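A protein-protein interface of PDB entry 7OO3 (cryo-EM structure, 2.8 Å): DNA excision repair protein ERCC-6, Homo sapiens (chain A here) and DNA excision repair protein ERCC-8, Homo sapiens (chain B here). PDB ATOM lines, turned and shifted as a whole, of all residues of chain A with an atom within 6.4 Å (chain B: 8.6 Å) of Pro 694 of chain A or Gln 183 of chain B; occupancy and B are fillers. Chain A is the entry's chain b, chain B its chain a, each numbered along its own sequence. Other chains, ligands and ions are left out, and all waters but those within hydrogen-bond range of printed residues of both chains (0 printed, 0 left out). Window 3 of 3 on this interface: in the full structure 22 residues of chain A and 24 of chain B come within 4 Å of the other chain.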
ATOM      1  N   ARG A 670       1.770 -21.055   5.793  1.00  0.00           N
ATOM      2  CA  ARG A 670       0.567 -21.787   6.180  1.00  0.00           C
ATOM      3  C   ARG A 670      -0.614 -21.171   5.448  1.00  0.00           C
ATOM      4  O   ARG A 670      -0.990 -20.028   5.726  1.00  0.00           O
ATOM      5  CB  ARG A 670       0.338 -21.727   7.688  1.00  0.00           C
ATOM      6  CG  ARG A 670       1.214 -22.640   8.524  1.00  0.00           C
ATOM      7  CD  ARG A 670       2.480 -21.935   8.965  1.00  0.00           C
ATOM      8  NE  ARG A 670       3.248 -22.738   9.908  1.00  0.00           N
ATOM      9  CZ  ARG A 670       2.934 -22.898  11.191  1.00  0.00           C
ATOM     10  NH1 ARG A 670       1.850 -22.329  11.706  1.00  0.00           N
ATOM     11  NH2 ARG A 670       3.705 -23.645  11.965  1.00  0.00           N
ATOM     12  N   TRP A 686     -10.265 -17.747  15.803  1.00  0.00           N
ATOM     13  CA  TRP A 686      -9.012 -17.717  16.542  1.00  0.00           C
ATOM     14  C   TRP A 686      -8.156 -18.928  16.221  1.00  0.00           C
ATOM     15  O   TRP A 686      -6.937 -18.808  16.088  1.00  0.00           O
ATOM     16  CB  TRP A 686      -9.249 -17.659  18.046  1.00  0.00           C
ATOM     17  CG  TRP A 686      -7.947 -17.525  18.768  1.00  0.00           C
ATOM     18  CD1 TRP A 686      -7.315 -16.369  19.100  1.00  0.00           C
ATOM     19  CD2 TRP A 686      -7.092 -18.588  19.206  1.00  0.00           C
ATOM     20  NE1 TRP A 686      -6.128 -16.641  19.726  1.00  0.00           N
ATOM     21  CE2 TRP A 686      -5.967 -17.998  19.803  1.00  0.00           C
ATOM     22  CE3 TRP A 686      -7.173 -19.980  19.150  1.00  0.00           C
ATOM     23  CZ2 TRP A 686      -4.932 -18.749  20.348  1.00  0.00           C
ATOM     24  CZ3 TRP A 686      -6.147 -20.725  19.691  1.00  0.00           C
ATOM     25  CH2 TRP A 686      -5.043 -20.110  20.285  1.00  0.00           C
ATOM     26  N   PHE A 689      -6.539 -18.535  12.782  1.00  0.00           N
ATOM     27  CA  PHE A 689      -5.476 -17.539  12.763  1.00  0.00           C
ATOM     28  C   PHE A 689      -4.279 -17.963  13.599  1.00  0.00           C
ATOM     29  O   PHE A 689      -3.143 -17.603  13.273  1.00  0.00           O
ATOM     30  CB  PHE A 689      -6.018 -16.192  13.202  1.00  0.00           C
ATOM     31  CG  PHE A 689      -6.516 -15.383  12.061  1.00  0.00           C
ATOM     32  CD1 PHE A 689      -5.650 -14.578  11.351  1.00  0.00           C
ATOM     33  CD2 PHE A 689      -7.824 -15.493  11.639  1.00  0.00           C
ATOM     34  CE1 PHE A 689      -6.092 -13.856  10.281  1.00  0.00           C
ATOM     35  CE2 PHE A 689      -8.269 -14.773  10.565  1.00  0.00           C
ATOM     36  CZ  PHE A 689      -7.400 -13.960   9.882  1.00  0.00           C
ATOM     37  N   ASP A 690      -4.501 -18.733  14.662  1.00  0.00           N
ATOM     38  CA  ASP A 690      -3.377 -19.314  15.378  1.00  0.00           C
ATOM     39  C   ASP A 690      -2.618 -20.282  14.488  1.00  0.00           C
ATOM     40  O   ASP A 690      -1.401 -20.432  14.636  1.00  0.00           O
ATOM     41  CB  ASP A 690      -3.864 -20.016  16.646  1.00  0.00           C
ATOM     42  CG  ASP A 690      -2.725 -20.561  17.492  1.00  0.00           C
ATOM     43  OD1 ASP A 690      -1.986 -21.451  17.022  1.00  0.00           O
ATOM     44  OD2 ASP A 690      -2.584 -20.118  18.650  1.00  0.00           O
ATOM     45  N   PHE A 691      -3.308 -20.939  13.556  1.00  0.00           N
ATOM     46  CA  PHE A 691      -2.586 -21.771  12.601  1.00  0.00           C
ATOM     47  C   PHE A 691      -1.751 -20.926  11.645  1.00  0.00           C
ATOM     48  O   PHE A 691      -0.526 -21.077  11.580  1.00  0.00           O
ATOM     49  CB  PHE A 691      -3.534 -22.657  11.803  1.00  0.00           C
ATOM     50  CG  PHE A 691      -2.822 -23.494  10.790  1.00  0.00           C
ATOM     51  CD1 PHE A 691      -1.926 -24.463  11.191  1.00  0.00           C
ATOM     52  CD2 PHE A 691      -2.991 -23.269   9.442  1.00  0.00           C
ATOM     53  CE1 PHE A 691      -1.248 -25.216  10.269  1.00  0.00           C
ATOM     54  CE2 PHE A 691      -2.315 -24.021   8.518  1.00  0.00           C
ATOM     55  CZ  PHE A 691      -1.438 -24.993   8.933  1.00  0.00           C
ATOM     56  N   ILE A 692      -2.392 -20.033  10.883  1.00  0.00           N
ATOM     57  CA  ILE A 692      -1.679 -19.412   9.764  1.00  0.00           C
ATOM     58  C   ILE A 692      -0.574 -18.488  10.264  1.00  0.00           C
ATOM     59  O   ILE A 692       0.486 -18.375   9.638  1.00  0.00           O
ATOM     60  CB  ILE A 692      -2.640 -18.663   8.821  1.00  0.00           C
ATOM     61  CG1 ILE A 692      -3.350 -17.518   9.545  1.00  0.00           C
ATOM     62  CG2 ILE A 692      -3.647 -19.639   8.230  1.00  0.00           C
ATOM     63  CD1 ILE A 692      -4.115 -16.602   8.653  1.00  0.00           C
ATOM     64  N   PHE A 693      -0.803 -17.808  11.385  1.00  0.00           N
ATOM     65  CA  PHE A 693       0.103 -16.769  11.873  1.00  0.00           C
ATOM     66  C   PHE A 693       0.085 -16.888  13.390  1.00  0.00           C
ATOM     67  O   PHE A 693      -0.850 -16.398  14.043  1.00  0.00           O
ATOM     68  CB  PHE A 693      -0.340 -15.379  11.422  1.00  0.00           C
ATOM     69  CG  PHE A 693       0.742 -14.339  11.481  1.00  0.00           C
ATOM     70  CD1 PHE A 693       1.366 -14.021  12.670  1.00  0.00           C
ATOM     71  CD2 PHE A 693       1.160 -13.705  10.326  1.00  0.00           C
ATOM     72  CE1 PHE A 693       2.365 -13.073  12.709  1.00  0.00           C
ATOM     73  CE2 PHE A 693       2.155 -12.755  10.363  1.00  0.00           C
ATOM     74  CZ  PHE A 693       2.756 -12.438  11.554  1.00  0.00           C
ATOM     75  N   PRO A 694       1.079 -17.554  13.991  1.00  0.00           N
ATOM     76  CA  PRO A 694       0.956 -17.891  15.420  1.00  0.00           C
ATOM     77  C   PRO A 694       0.764 -16.694  16.334  1.00  0.00           C
ATOM     78  O   PRO A 694       0.070 -16.817  17.350  1.00  0.00           O
ATOM     79  CB  PRO A 694       2.277 -18.612  15.717  1.00  0.00           C
ATOM     80  CG  PRO A 694       2.692 -19.176  14.425  1.00  0.00           C
ATOM     81  CD  PRO A 694       2.281 -18.170  13.401  1.00  0.00           C
ATOM     82  N   GLY A 695       1.344 -15.542  16.004  1.00  0.00           N
ATOM     83  CA  GLY A 695       1.375 -14.429  16.932  1.00  0.00           C
ATOM     84  C   GLY A 695       0.402 -13.293  16.685  1.00  0.00           C
ATOM     85  O   GLY A 695       0.205 -12.467  17.579  1.00  0.00           O
ATOM     86  N   LYS A 696      -0.217 -13.226  15.505  1.00  0.00           N
ATOM     87  CA  LYS A 696      -0.971 -12.033  15.129  1.00  0.00           C
ATOM     88  C   LYS A 696      -2.139 -11.772  16.070  1.00  0.00           C
ATOM     89  O   LYS A 696      -2.154 -10.757  16.770  1.00  0.00           O
ATOM     90  CB  LYS A 696      -1.467 -12.144  13.686  1.00  0.00           C
ATOM     91  CG  LYS A 696      -2.295 -10.961  13.176  1.00  0.00           C
ATOM     92  CD  LYS A 696      -1.513  -9.648  13.156  1.00  0.00           C
ATOM     93  CE  LYS A 696      -0.584  -9.551  11.963  1.00  0.00           C
ATOM     94  NZ  LYS A 696      -0.268  -8.140  11.630  1.00  0.00           N
ATOM     95  N   LEU A 697      -3.137 -12.647  16.087  1.00  0.00           N
ATOM     96  CA  LEU A 697      -4.126 -12.571  17.150  1.00  0.00           C
ATOM     97  C   LEU A 697      -3.526 -13.098  18.447  1.00  0.00           C
ATOM     98  O   LEU A 697      -2.691 -14.005  18.449  1.00  0.00           O
ATOM     99  CB  LEU A 697      -5.388 -13.349  16.784  1.00  0.00           C
ATOM    100  CG  LEU A 697      -6.181 -12.842  15.574  1.00  0.00           C
ATOM    101  CD1 LEU A 697      -7.401 -13.715  15.360  1.00  0.00           C
ATOM    102  CD2 LEU A 697      -6.599 -11.383  15.713  1.00  0.00           C
ATOM    103  N   GLY A 698      -3.953 -12.515  19.558  1.00  0.00           N
ATOM    104  CA  GLY A 698      -3.382 -12.845  20.843  1.00  0.00           C
ATOM    105  C   GLY A 698      -3.737 -14.253  21.273  1.00  0.00           C
ATOM    106  O   GLY A 698      -4.411 -15.011  20.577  1.00  0.00           O
ATOM    107  N   PRO B 166       6.564 -12.106  29.038  1.00  0.00           N
ATOM    108  CA  PRO B 166       7.628 -12.585  28.147  1.00  0.00           C
ATOM    109  C   PRO B 166       7.399 -12.261  26.683  1.00  0.00           C
ATOM    110  O   PRO B 166       8.274 -12.563  25.861  1.00  0.00           O
ATOM    111  CB  PRO B 166       7.622 -14.104  28.371  1.00  0.00           C
ATOM    112  CG  PRO B 166       6.720 -14.344  29.529  1.00  0.00           C
ATOM    113  CD  PRO B 166       5.746 -13.231  29.519  1.00  0.00           C
ATOM    114  N   LYS B 167       6.258 -11.681  26.331  1.00  0.00           N
ATOM    115  CA  LYS B 167       5.898 -11.400  24.951  1.00  0.00           C
ATOM    116  C   LYS B 167       6.083  -9.919  24.644  1.00  0.00           C
ATOM    117  O   LYS B 167       5.899  -9.060  25.509  1.00  0.00           O
ATOM    118  CB  LYS B 167       4.449 -11.806  24.694  1.00  0.00           C
ATOM    119  CG  LYS B 167       4.209 -13.300  24.764  1.00  0.00           C
ATOM    120  CD  LYS B 167       2.831 -13.609  25.322  1.00  0.00           C
ATOM    121  CE  LYS B 167       2.482 -15.076  25.158  1.00  0.00           C
ATOM    122  NZ  LYS B 167       3.509 -15.965  25.769  1.00  0.00           N
ATOM    123  N   VAL B 168       6.439  -9.628  23.398  1.00  0.00           N
ATOM    124  CA  VAL B 168       6.604  -8.262  22.917  1.00  0.00           C
ATOM    125  C   VAL B 168       5.312  -7.865  22.228  1.00  0.00           C
ATOM    126  O   VAL B 168       4.912  -8.496  21.247  1.00  0.00           O
ATOM    127  CB  VAL B 168       7.796  -8.137  21.955  1.00  0.00           C
ATOM    128  CG1 VAL B 168       8.032  -6.681  21.579  1.00  0.00           C
ATOM    129  CG2 VAL B 168       9.047  -8.726  22.564  1.00  0.00           C
ATOM    130  N   GLN B 169       4.671  -6.811  22.714  1.00  0.00           N
ATOM    131  CA  GLN B 169       3.413  -6.352  22.144  1.00  0.00           C
ATOM    132  C   GLN B 169       3.699  -5.402  20.992  1.00  0.00           C
ATOM    133  O   GLN B 169       4.574  -4.546  21.101  1.00  0.00           O
ATOM    134  CB  GLN B 169       2.553  -5.645  23.195  1.00  0.00           C
ATOM    135  CG  GLN B 169       2.467  -6.316  24.573  1.00  0.00           C
ATOM    136  CD  GLN B 169       1.413  -7.397  24.644  1.00  0.00           C
ATOM    137  OE1 GLN B 169       1.704  -8.535  25.003  1.00  0.00           O
ATOM    138  NE2 GLN B 169       0.175  -7.043  24.322  1.00  0.00           N
ATOM    139  N   SER B 179      -2.948  -6.686  19.445  1.00  0.00           N
ATOM    140  CA  SER B 179      -3.033  -8.123  19.672  1.00  0.00           C
ATOM    141  C   SER B 179      -1.751  -8.853  19.295  1.00  0.00           C
ATOM    142  O   SER B 179      -1.412  -9.860  19.924  1.00  0.00           O
ATOM    143  CB  SER B 179      -4.207  -8.707  18.884  1.00  0.00           C
ATOM    144  OG  SER B 179      -4.105  -8.386  17.511  1.00  0.00           O
ATOM    145  N   HIS B 180      -1.042  -8.371  18.277  1.00  0.00           N
ATOM    146  CA  HIS B 180       0.159  -9.044  17.797  1.00  0.00           C
ATOM    147  C   HIS B 180       1.182  -9.169  18.913  1.00  0.00           C
ATOM    148  O   HIS B 180       1.436  -8.212  19.648  1.00  0.00           O
ATOM    149  CB  HIS B 180       0.759  -8.266  16.630  1.00  0.00           C
ATOM    150  CG  HIS B 180       1.783  -9.034  15.854  1.00  0.00           C
ATOM    151  ND1 HIS B 180       2.996  -9.408  16.386  1.00  0.00           N
ATOM    152  CD2 HIS B 180       1.795  -9.450  14.567  1.00  0.00           C
ATOM    153  CE1 HIS B 180       3.694 -10.055  15.472  1.00  0.00           C
ATOM    154  NE2 HIS B 180       2.990 -10.091  14.359  1.00  0.00           N
ATOM    155  N   ILE B 181       1.766 -10.357  19.040  1.00  0.00           N
ATOM    156  CA  ILE B 181       2.772 -10.632  20.058  1.00  0.00           C
ATOM    157  C   ILE B 181       3.909 -11.416  19.426  1.00  0.00           C
ATOM    158  O   ILE B 181       3.682 -12.335  18.632  1.00  0.00           O
ATOM    159  CB  ILE B 181       2.193 -11.402  21.261  1.00  0.00           C
ATOM    160  CG1 ILE B 181       1.361 -12.597  20.793  1.00  0.00           C
ATOM    161  CG2 ILE B 181       1.372 -10.472  22.130  1.00  0.00           C
ATOM    162  CD1 ILE B 181       1.072 -13.600  21.882  1.00  0.00           C
ATOM    163  N   LEU B 182       5.132 -11.040  19.770  1.00  0.00           N
ATOM    164  CA  LEU B 182       6.330 -11.766  19.371  1.00  0.00           C
ATOM    165  C   LEU B 182       6.790 -12.572  20.577  1.00  0.00           C
ATOM    166  O   LEU B 182       7.250 -12.000  21.569  1.00  0.00           O
ATOM    167  CB  LEU B 182       7.423 -10.810  18.900  1.00  0.00           C
ATOM    168  CG  LEU B 182       7.035  -9.731  17.890  1.00  0.00           C
ATOM    169  CD1 LEU B 182       8.012  -8.580  17.954  1.00  0.00           C
ATOM    170  CD2 LEU B 182       7.009 -10.315  16.495  1.00  0.00           C
ATOM    171  N   GLN B 183       6.662 -13.892  20.493  1.00  0.00           N
ATOM    172  CA  GLN B 183       6.989 -14.783  21.592  1.00  0.00           C
ATOM    173  C   GLN B 183       8.288 -15.517  21.300  1.00  0.00           C
ATOM    174  O   GLN B 183       8.605 -15.822  20.148  1.00  0.00           O
ATOM    175  CB  GLN B 183       5.847 -15.777  21.859  1.00  0.00           C
ATOM    176  CG  GLN B 183       5.598 -16.852  20.798  1.00  0.00           C
ATOM    177  CD  GLN B 183       4.713 -16.365  19.669  1.00  0.00           C
ATOM    178  OE1 GLN B 183       4.518 -15.165  19.490  1.00  0.00           O
ATOM    179  NE2 GLN B 183       4.160 -17.302  18.907  1.00  0.00           N
ATOM    180  N   GLY B 184       9.028 -15.812  22.362  1.00  0.00           N
ATOM    181  CA  GLY B 184      10.348 -16.393  22.240  1.00  0.00           C
ATOM    182  C   GLY B 184      11.284 -15.945  23.341  1.00  0.00           C
ATOM    183  O   GLY B 184      12.271 -16.626  23.628  1.00  0.00           O
ATOM    184  N   HIS B 185      10.981 -14.821  23.981  1.00  0.00           N
ATOM    185  CA  HIS B 185      11.669 -14.465  25.210  1.00  0.00           C
ATOM    186  C   HIS B 185      11.028 -15.193  26.384  1.00  0.00           C
ATOM    187  O   HIS B 185       9.923 -15.729  26.289  1.00  0.00           O
ATOM    188  CB  HIS B 185      11.646 -12.954  25.427  1.00  0.00           C
ATOM    189  CG  HIS B 185      12.759 -12.228  24.738  1.00  0.00           C
ATOM    190  ND1 HIS B 185      14.073 -12.635  24.818  1.00  0.00           N
ATOM    191  CD2 HIS B 185      12.756 -11.123  23.958  1.00  0.00           C
ATOM    192  CE1 HIS B 185      14.830 -11.811  24.118  1.00  0.00           C
ATOM    193  NE2 HIS B 185      14.056 -10.885  23.588  1.00  0.00           N
ATOM    194  N   ARG B 186      11.738 -15.200  27.510  1.00  0.00           N
ATOM    195  CA  ARG B 186      11.332 -15.958  28.681  1.00  0.00           C
ATOM    196  C   ARG B 186      11.136 -15.108  29.923  1.00  0.00           C
ATOM    197  O   ARG B 186      10.604 -15.617  30.915  1.00  0.00           O
ATOM    198  CB  ARG B 186      12.375 -17.042  28.992  1.00  0.00           C
ATOM    199  CG  ARG B 186      12.341 -18.221  28.039  1.00  0.00           C
ATOM    200  CD  ARG B 186      13.231 -19.397  28.462  1.00  0.00           C
ATOM    201  NE  ARG B 186      14.659 -19.175  28.224  1.00  0.00           N
ATOM    202  CZ  ARG B 186      15.482 -18.480  29.011  1.00  0.00           C
ATOM    203  NH1 ARG B 186      15.066 -17.945  30.152  1.00  0.00           N
ATOM    204  NH2 ARG B 186      16.756 -18.352  28.667  1.00  0.00           N
ATOM    205  N   ILE B 189      10.783  -8.067  28.998  1.00  0.00           N
ATOM    206  CA  ILE B 189      11.494  -7.364  27.938  1.00  0.00           C
ATOM    207  C   ILE B 189      11.777  -5.954  28.436  1.00  0.00           C
ATOM    208  O   ILE B 189      10.863  -5.146  28.599  1.00  0.00           O
ATOM    209  CB  ILE B 189      10.707  -7.353  26.623  1.00  0.00           C
ATOM    210  CG1 ILE B 189      10.515  -8.777  26.102  1.00  0.00           C
ATOM    211  CG2 ILE B 189      11.421  -6.529  25.555  1.00  0.00           C
ATOM    212  CD1 ILE B 189       9.294  -9.467  26.594  1.00  0.00           C
ATOM    213  N   THR B 204      14.825  -6.648  20.495  1.00  0.00           N
ATOM    214  CA  THR B 204      14.190  -6.681  21.802  1.00  0.00           C
ATOM    215  C   THR B 204      15.130  -7.370  22.775  1.00  0.00           C
ATOM    216  O   THR B 204      15.646  -8.453  22.486  1.00  0.00           O
ATOM    217  CB  THR B 204      12.838  -7.401  21.748  1.00  0.00           C
ATOM    218  OG1 THR B 204      13.042  -8.783  21.457  1.00  0.00           O
ATOM    219  CG2 THR B 204      11.965  -6.820  20.651  1.00  0.00           C
ATOM    220  N   LYS B 212      16.979 -10.486  20.850  1.00  0.00           N
ATOM    221  CA  LYS B 212      16.473 -11.112  19.642  1.00  0.00           C
ATOM    222  C   LYS B 212      16.125 -10.044  18.624  1.00  0.00           C
ATOM    223  O   LYS B 212      15.568  -9.000  18.969  1.00  0.00           O
ATOM    224  CB  LYS B 212      15.253 -11.972  19.952  1.00  0.00           C
ATOM    225  CG  LYS B 212      15.599 -13.196  20.769  1.00  0.00           C
ATOM    226  CD  LYS B 212      14.398 -14.072  21.013  1.00  0.00           C
ATOM    227  CE  LYS B 212      14.796 -15.332  21.750  1.00  0.00           C
ATOM    228  NZ  LYS B 212      15.119 -16.446  20.821  1.00  0.00           N
ATOM    229  N   TRP B 214      13.813  -9.439  15.375  1.00  0.00           N
ATOM    230  CA  TRP B 214      12.596  -9.950  14.785  1.00  0.00           C
ATOM    231  C   TRP B 214      12.346  -9.226  13.478  1.00  0.00           C
ATOM    232  O   TRP B 214      12.747  -8.075  13.295  1.00  0.00           O
ATOM    233  CB  TRP B 214      11.384  -9.734  15.695  1.00  0.00           C
ATOM    234  CG  TRP B 214      11.591 -10.086  17.118  1.00  0.00           C
ATOM    235  CD1 TRP B 214      12.223  -9.337  18.061  1.00  0.00           C
ATOM    236  CD2 TRP B 214      11.142 -11.267  17.778  1.00  0.00           C
ATOM    237  NE1 TRP B 214      12.207  -9.982  19.267  1.00  0.00           N
ATOM    238  CE2 TRP B 214      11.547 -11.172  19.120  1.00  0.00           C
ATOM    239  CE3 TRP B 214      10.441 -12.400  17.365  1.00  0.00           C
ATOM    240  CZ2 TRP B 214      11.275 -12.165  20.051  1.00  0.00           C
ATOM    241  CZ3 TRP B 214      10.173 -13.383  18.287  1.00  0.00           C
ATOM    242  CH2 TRP B 214      10.589 -13.261  19.615  1.00  0.00           C
ATOM    243  N   ARG B 217       7.028  -8.696  10.132  1.00  0.00           N
ATOM    244  CA  ARG B 217       6.254  -9.309   9.059  1.00  0.00           C
ATOM    245  C   ARG B 217       6.271 -10.823   9.173  1.00  0.00           C
ATOM    246  O   ARG B 217       5.251 -11.484   8.953  1.00  0.00           O
ATOM    247  CB  ARG B 217       6.819  -8.905   7.702  1.00  0.00           C
ATOM    248  CG  ARG B 217       6.839  -7.426   7.427  1.00  0.00           C
ATOM    249  CD  ARG B 217       7.376  -7.130   6.033  1.00  0.00           C
ATOM    250  NE  ARG B 217       8.694  -7.722   5.795  1.00  0.00           N
ATOM    251  CZ  ARG B 217       9.594  -7.260   4.930  1.00  0.00           C
ATOM    252  NH1 ARG B 217       9.348  -6.191   4.182  1.00  0.00           N
ATOM    253  NH2 ARG B 217      10.755  -7.885   4.806  1.00  0.00           N
ATOM    254  N   ARG B 218       7.426 -11.383   9.509  1.00  0.00           N
ATOM    255  CA  ARG B 218       7.605 -12.823   9.518  1.00  0.00           C
ATOM    256  C   ARG B 218       6.716 -13.462  10.575  1.00  0.00           C
ATOM    257  O   ARG B 218       6.419 -12.867  11.614  1.00  0.00           O
ATOM    258  CB  ARG B 218       9.072 -13.155   9.777  1.00  0.00           C
ATOM    259  CG  ARG B 218       9.459 -14.593   9.466  1.00  0.00           C
ATOM    260  CD  ARG B 218      10.934 -14.768   9.073  1.00  0.00           C
ATOM    261  NE  ARG B 218      11.398 -13.804   8.075  1.00  0.00           N
ATOM    262  CZ  ARG B 218      12.617 -13.791   7.543  1.00  0.00           C
ATOM    263  NH1 ARG B 218      13.522 -14.698   7.892  1.00  0.00           N
ATOM    264  NH2 ARG B 218      12.933 -12.868   6.646  1.00  0.00           N
ATOM    265  N   ALA B 219       6.284 -14.689  10.295  1.00  0.00           N
ATOM    266  CA  ALA B 219       5.411 -15.447  11.180  1.00  0.00           C
ATOM    267  C   ALA B 219       6.117 -16.659  11.779  1.00  0.00           C
ATOM    268  O   ALA B 219       5.467 -17.644  12.131  1.00  0.00           O
ATOM    269  CB  ALA B 219       4.159 -15.890  10.427  1.00  0.00           C
ATOM    270  N   SER B 220       7.447 -16.593  11.913  1.00  0.00           N
ATOM    271  CA  SER B 220       8.232 -17.755  12.314  1.00  0.00           C
ATOM    272  C   SER B 220       9.311 -17.393  13.328  1.00  0.00           C
ATOM    273  O   SER B 220      10.399 -17.979  13.313  1.00  0.00           O
ATOM    274  CB  SER B 220       8.877 -18.421  11.100  1.00  0.00           C
ATOM    275  OG  SER B 220       9.830 -17.564  10.498  1.00  0.00           O
ATOM    276  N   GLY B 221       9.035 -16.441  14.211  1.00  0.00           N
ATOM    277  CA  GLY B 221       9.929 -16.182  15.318  1.00  0.00           C
ATOM    278  C   GLY B 221      11.080 -15.259  14.967  1.00  0.00           C
ATOM    279  O   GLY B 221      11.151 -14.655  13.894  1.00  0.00           O
ATOM    280  N   CYS B 222      12.001 -15.156  15.920  1.00  0.00           N
ATOM    281  CA  CYS B 222      13.096 -14.204  15.813  1.00  0.00           C
ATOM    282  C   CYS B 222      14.031 -14.562  14.667  1.00  0.00           C
ATOM    283  O   CYS B 222      14.272 -15.737  14.379  1.00  0.00           O
ATOM    284  CB  CYS B 222      13.871 -14.143  17.129  1.00  0.00           C
ATOM    285  SG  CYS B 222      14.841 -15.615  17.540  1.00  0.00           S
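Among the printed residues, pairs that only touch across the chains: Phe 693 of chain A with His 180 of chain B (3.5 Å), Phe 693 of chain A with Arg 217 of chain B (3.6 Å), Phe 693 of chain A with Arg 218 of chain B (3.7 Å), Phe 693 of chain A with Ala 219 of chain B (3.7 Å), Pro 694 of chain A with Gln 183 of chain B (3.9 Å), Pro 694 of chain A with Ala 219 of chain B (3.5 Å), Gly 695 of chain A with Ser 179 of chain B (3.9 Å), Gly 695 of chain A with His 180 of chain B (3.4 Å) and Gly 698 of chain A with Ser 179 of chain B (3.7 Å).
The side-chain amide oxygen (OE1) of Gln 183 of chain B sits close to the backbone carbonyl oxygen (O) of Ile 181 of chain B, at 3.1 Å.
The indole nitrogen (NE1) of Trp 686 of chain A sits at hydrogen-bond distance from the backbone carbonyl oxygen (O) of Gly 698 of chain A (2.5 Å).
OG of Ser 179 of chain B sits at hydrogen-bond distance from O of Lys 696 of chain A, at 3.2 Å.
N of His 180 of chain B lies within hydrogen-bond range of O of Lys 696 of chain A, at 3.0 Å.
N of Ile 181 of chain B sits at hydrogen-bond distance from O of Gly 695 of chain A (3.0 Å).
Of the 12 printed residues of chain A, 5 touch a printed residue of chain B.
Hydrophobic or aromatic side chains of chain A within 4 Å of the printed part of chain B: Phe 693 and Pro 694.
Along chain A the printed residues that touch a printed residue of chain B span positions 693 to 698.
Hydrophobic or aromatic side chains of chain B that line the printed part of chain A: His 180, Ile 181 and Ala 219.
Among the printed residues, 12 pairs touch across the chains.
Printed residues of chain B within 4 Å of Phe 693 of chain A: His 180, Arg 217, Arg 218 and Ala 219.
Of chain B, only Gln 183 and Ala 219 come within 4 Å of Pro 694 of chain A.
Of chain B, only Ser 179, His 180 and Ile 181 come within 4 Å of Gly 695 of chain A.
Printed residues of chain B within 4 Å of Gly 698 of chain A: Ser 179 (3.7 Å).
Of the printed residues of chain A, Ser 179 of chain B touches Gly 695, Lys 696 and Gly 698.
Of chain A, only Pro 694 (3.9 Å) comes within 4 Å of Gln 183 of chain B.
Of the printed residues of chain A, Arg 217 of chain B touches Phe 693.
Of the printed residues of chain A, Ala 219 of chain B touches Phe 693 (3.7 Å) and Pro 694 (3.5 Å).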
